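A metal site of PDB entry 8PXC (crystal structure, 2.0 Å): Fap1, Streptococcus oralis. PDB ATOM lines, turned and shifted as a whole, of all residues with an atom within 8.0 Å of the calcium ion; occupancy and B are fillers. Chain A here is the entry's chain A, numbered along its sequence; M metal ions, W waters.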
ATOM      1  N   ALA A 278      21.388  13.113 -17.156  1.00  0.00           N
ATOM      2  CA  ALA A 278      21.161  14.545 -17.097  1.00  0.00           C
ATOM      3  C   ALA A 278      20.407  14.941 -18.370  1.00  0.00           C
ATOM      4  O   ALA A 278      20.588  14.352 -19.429  1.00  0.00           O
ATOM      5  CB  ALA A 278      22.453  15.270 -16.972  1.00  0.00           C
ATOM      6  N   GLN A 279      19.544  15.941 -18.255  1.00  0.00           N
ATOM      7  CA  GLN A 279      18.813  16.429 -19.437  1.00  0.00           C
ATOM      8  C   GLN A 279      19.782  16.961 -20.505  1.00  0.00           C
ATOM      9  O   GLN A 279      19.480  16.825 -21.680  1.00  0.00           O
ATOM     10  CB  GLN A 279      17.791  17.492 -19.040  1.00  0.00           C
ATOM     11  CG  GLN A 279      16.536  16.892 -18.374  1.00  0.00           C
ATOM     12  CD  GLN A 279      15.552  17.987 -18.030  1.00  0.00           C
ATOM     13  OE1 GLN A 279      15.784  18.784 -17.138  1.00  0.00           O
ATOM     14  NE2 GLN A 279      14.451  18.035 -18.782  1.00  0.00           N
ATOM     15  N   SER A 280      20.946  17.501 -20.084  1.00  0.00           N
ATOM     16  CA  SER A 280      21.964  17.970 -21.018  1.00  0.00           C
ATOM     17  C   SER A 280      22.431  16.847 -21.939  1.00  0.00           C
ATOM     18  O   SER A 280      22.861  17.133 -23.043  1.00  0.00           O
ATOM     19  CB  SER A 280      23.126  18.626 -20.362  1.00  0.00           C
ATOM     20  OG  SER A 280      23.757  17.701 -19.482  1.00  0.00           O
ATOM     21  N   GLU A 281      22.298  15.602 -21.546  1.00  0.00           N
ATOM     22  CA  GLU A 281      22.690  14.499 -22.426  1.00  0.00           C
ATOM     23  C   GLU A 281      21.678  14.349 -23.568  1.00  0.00           C
ATOM     24  O   GLU A 281      22.052  13.875 -24.639  1.00  0.00           O
ATOM     25  CB  GLU A 281      22.793  13.181 -21.675  1.00  0.00           C
ATOM     26  CG  GLU A 281      23.759  13.233 -20.527  1.00  0.00           C
ATOM     27  CD  GLU A 281      23.749  11.941 -19.701  1.00  0.00           C
ATOM     28  OE1 GLU A 281      23.690  10.828 -20.369  1.00  0.00           O
ATOM     29  OE2 GLU A 281      23.803  12.023 -18.409  1.00  0.00           O
ATOM     30  N   LYS A 282      20.410  14.719 -23.328  1.00  0.00           N
ATOM     31  CA  LYS A 282      19.363  14.498 -24.318  1.00  0.00           C
ATOM     32  C   LYS A 282      19.332  15.599 -25.375  1.00  0.00           C
ATOM     33  O   LYS A 282      19.035  15.308 -26.534  1.00  0.00           O
ATOM     34  CB  LYS A 282      17.995  14.359 -23.619  1.00  0.00           C
ATOM     35  CG  LYS A 282      16.787  14.339 -24.550  1.00  0.00           C
ATOM     36  CD  LYS A 282      15.483  14.039 -23.840  1.00  0.00           C
ATOM     37  CE  LYS A 282      14.280  14.206 -24.736  1.00  0.00           C
ATOM     38  NZ  LYS A 282      13.019  13.800 -24.064  1.00  0.00           N
ATOM     39  N   TYR A 283      19.531  16.861 -24.978  1.00  0.00           N
ATOM     40  CA  TYR A 283      19.225  17.993 -25.835  1.00  0.00           C
ATOM     41  C   TYR A 283      20.492  18.546 -26.508  1.00  0.00           C
ATOM     42  O   TYR A 283      21.638  18.428 -26.039  1.00  0.00           O
ATOM     43  CB  TYR A 283      18.451  19.043 -25.039  1.00  0.00           C
ATOM     44  CG  TYR A 283      17.135  18.533 -24.511  1.00  0.00           C
ATOM     45  CD1 TYR A 283      16.032  18.395 -25.327  1.00  0.00           C
ATOM     46  CD2 TYR A 283      16.993  18.137 -23.192  1.00  0.00           C
ATOM     47  CE1 TYR A 283      14.836  17.855 -24.865  1.00  0.00           C
ATOM     48  CE2 TYR A 283      15.811  17.601 -22.712  1.00  0.00           C
ATOM     49  CZ  TYR A 283      14.713  17.467 -23.543  1.00  0.00           C
ATOM     50  OH  TYR A 283      13.550  16.938 -23.073  1.00  0.00           O
ATOM     51  N   GLU A 284      20.254  19.143 -27.670  1.00  0.00           N
ATOM     52  CA  GLU A 284      21.297  19.785 -28.440  1.00  0.00           C
ATOM     53  C   GLU A 284      20.842  21.177 -28.882  1.00  0.00           C
ATOM     54  O   GLU A 284      20.151  21.329 -29.899  1.00  0.00           O
ATOM     55  CB  GLU A 284      21.676  18.957 -29.650  1.00  0.00           C
ATOM     56  CG  GLU A 284      22.806  19.592 -30.422  1.00  0.00           C
ATOM     57  CD  GLU A 284      23.163  18.899 -31.730  1.00  0.00           C
ATOM     58  OE1 GLU A 284      22.818  17.692 -31.874  1.00  0.00           O
ATOM     59  OE2 GLU A 284      23.818  19.543 -32.577  1.00  0.00           O
ATOM     60  N   PRO A 285      21.176  22.239 -28.108  1.00  0.00           N
ATOM     61  CA  PRO A 285      20.893  23.603 -28.558  1.00  0.00           C
ATOM     62  C   PRO A 285      21.617  23.960 -29.858  1.00  0.00           C
ATOM     63  O   PRO A 285      22.642  23.377 -30.187  1.00  0.00           O
ATOM     64  CB  PRO A 285      21.386  24.485 -27.414  1.00  0.00           C
ATOM     65  CG  PRO A 285      21.445  23.532 -26.211  1.00  0.00           C
ATOM     66  CD  PRO A 285      21.858  22.198 -26.797  1.00  0.00           C
ATOM     67  N   LEU A 322      13.464  21.705 -26.966  1.00  0.00           N
ATOM     68  CA  LEU A 322      14.016  21.910 -25.635  1.00  0.00           C
ATOM     69  C   LEU A 322      12.857  21.918 -24.623  1.00  0.00           C
ATOM     70  O   LEU A 322      11.734  22.329 -24.955  1.00  0.00           O
ATOM     71  CB  LEU A 322      14.833  23.202 -25.581  1.00  0.00           C
ATOM     72  CG  LEU A 322      15.946  23.305 -26.605  1.00  0.00           C
ATOM     73  CD1 LEU A 322      16.777  24.561 -26.403  1.00  0.00           C
ATOM     74  CD2 LEU A 322      16.858  22.099 -26.599  1.00  0.00           C
ATOM     75  N   VAL A 356      22.414  27.174 -21.761  1.00  0.00           N
ATOM     76  CA  VAL A 356      21.102  26.607 -21.628  1.00  0.00           C
ATOM     77  C   VAL A 356      21.100  25.746 -20.353  1.00  0.00           C
ATOM     78  O   VAL A 356      21.846  24.766 -20.270  1.00  0.00           O
ATOM     79  CB  VAL A 356      20.754  25.791 -22.885  1.00  0.00           C
ATOM     80  CG1 VAL A 356      19.371  25.160 -22.777  1.00  0.00           C
ATOM     81  CG2 VAL A 356      20.856  26.629 -24.168  1.00  0.00           C
ATOM     82  N   TYR A 358      18.799  23.412 -18.176  1.00  0.00           N
ATOM     83  CA  TYR A 358      17.578  22.633 -18.207  1.00  0.00           C
ATOM     84  C   TYR A 358      16.853  22.704 -16.866  1.00  0.00           C
ATOM     85  O   TYR A 358      17.428  23.075 -15.831  1.00  0.00           O
ATOM     86  CB  TYR A 358      17.892  21.207 -18.702  1.00  0.00           C
ATOM     87  CG  TYR A 358      18.504  21.223 -20.073  1.00  0.00           C
ATOM     88  CD1 TYR A 358      17.752  21.573 -21.179  1.00  0.00           C
ATOM     89  CD2 TYR A 358      19.876  21.063 -20.242  1.00  0.00           C
ATOM     90  CE1 TYR A 358      18.321  21.670 -22.442  1.00  0.00           C
ATOM     91  CE2 TYR A 358      20.474  21.178 -21.489  1.00  0.00           C
ATOM     92  CZ  TYR A 358      19.673  21.454 -22.615  1.00  0.00           C
ATOM     93  OH  TYR A 358      20.206  21.596 -23.866  1.00  0.00           O
ATOM     94  N   SER A 362      21.253  20.740 -15.155  1.00  0.00           N
ATOM     95  CA  SER A 362      22.354  20.459 -16.059  1.00  0.00           C
ATOM     96  C   SER A 362      22.358  21.503 -17.176  1.00  0.00           C
ATOM     97  O   SER A 362      21.344  22.199 -17.371  1.00  0.00           O
ATOM     98  CB  SER A 362      22.280  19.026 -16.610  1.00  0.00           C
ATOM     99  OG  SER A 362      21.144  18.885 -17.457  1.00  0.00           O
ATOM    100  N   THR A 363      23.507  21.626 -17.883  1.00  0.00           N
ATOM    101  CA  THR A 363      23.695  22.730 -18.815  1.00  0.00           C
ATOM    102  C   THR A 363      24.374  22.278 -20.104  1.00  0.00           C
ATOM    103  O   THR A 363      25.208  21.364 -20.092  1.00  0.00           O
ATOM    104  CB  THR A 363      24.503  23.900 -18.257  1.00  0.00           C
ATOM    105  OG1 THR A 363      25.852  23.466 -18.028  1.00  0.00           O
ATOM    106  CG2 THR A 363      24.007  24.458 -16.948  1.00  0.00           C
ATOM    107  N   ASP A 364      23.921  22.905 -21.210  1.00  0.00           N
ATOM    108  CA  ASP A 364      24.716  22.960 -22.421  1.00  0.00           C
ATOM    109  C   ASP A 364      25.294  24.389 -22.562  1.00  0.00           C
ATOM    110  O   ASP A 364      24.728  25.335 -22.055  1.00  0.00           O
ATOM    111  CB  ASP A 364      23.904  22.528 -23.642  1.00  0.00           C
ATOM    112  CG  ASP A 364      23.764  21.027 -23.835  1.00  0.00           C
ATOM    113  OD1 ASP A 364      24.812  20.354 -23.749  1.00  0.00           O
ATOM    114  OD2 ASP A 364      22.617  20.532 -24.035  1.00  0.00           O
ATOM    115  N   GLU A 365      26.419  24.510 -23.266  1.00  0.00           N
ATOM    116  CA  GLU A 365      27.060  25.767 -23.597  1.00  0.00           C
ATOM    117  C   GLU A 365      27.311  25.757 -25.094  1.00  0.00           C
ATOM    118  O   GLU A 365      27.790  24.781 -25.622  1.00  0.00           O
ATOM    119  CB  GLU A 365      28.392  25.982 -22.841  1.00  0.00           C
ATOM    120  CG  GLU A 365      28.197  26.080 -21.350  1.00  0.00           C
ATOM    121  CD  GLU A 365      29.412  26.480 -20.523  1.00  0.00           C
ATOM    122  OE1 GLU A 365      30.543  26.550 -21.054  1.00  0.00           O
ATOM    123  OE2 GLU A 365      29.181  26.758 -19.301  1.00  0.00           O
HETATM  124 CA    CA M   1      23.706  18.484 -24.802  1.00  0.00          CA
HETATM  125  O   HOH W   1      23.911  16.263 -26.074  1.00  0.00           O
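The backbone NH (N) of Ser 280 lies within hydrogen-bond range of the side-chain hydroxyl (OG) of Ser 362, 3.0 Å away. OD2 of Asp 364 sits close to OH of Tyr 358 (2.6 Å). The side-chain amino group (NZ) of Lys 282 sits close to the side-chain hydroxyl (OH) of Tyr 283 (3.3 Å). N of Asp 364 lies within hydrogen-bond range of O of Val 356 (2.9 Å).
The calcium ion is bound by O of Ser 280 (2.4 Å), O of Tyr 283 (2.4 Å), OD1 of Asp 364 (2.4 Å), OD2 of Asp 364 (2.4 Å) and water W1 (2.6 Å).
Three residues have an atom within 4 Å of the calcium ion: Ser 280, Tyr 283 and Asp 364. The nearest printed residue that does not touch the calcium ion is Glu 284 (4.5 Å).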
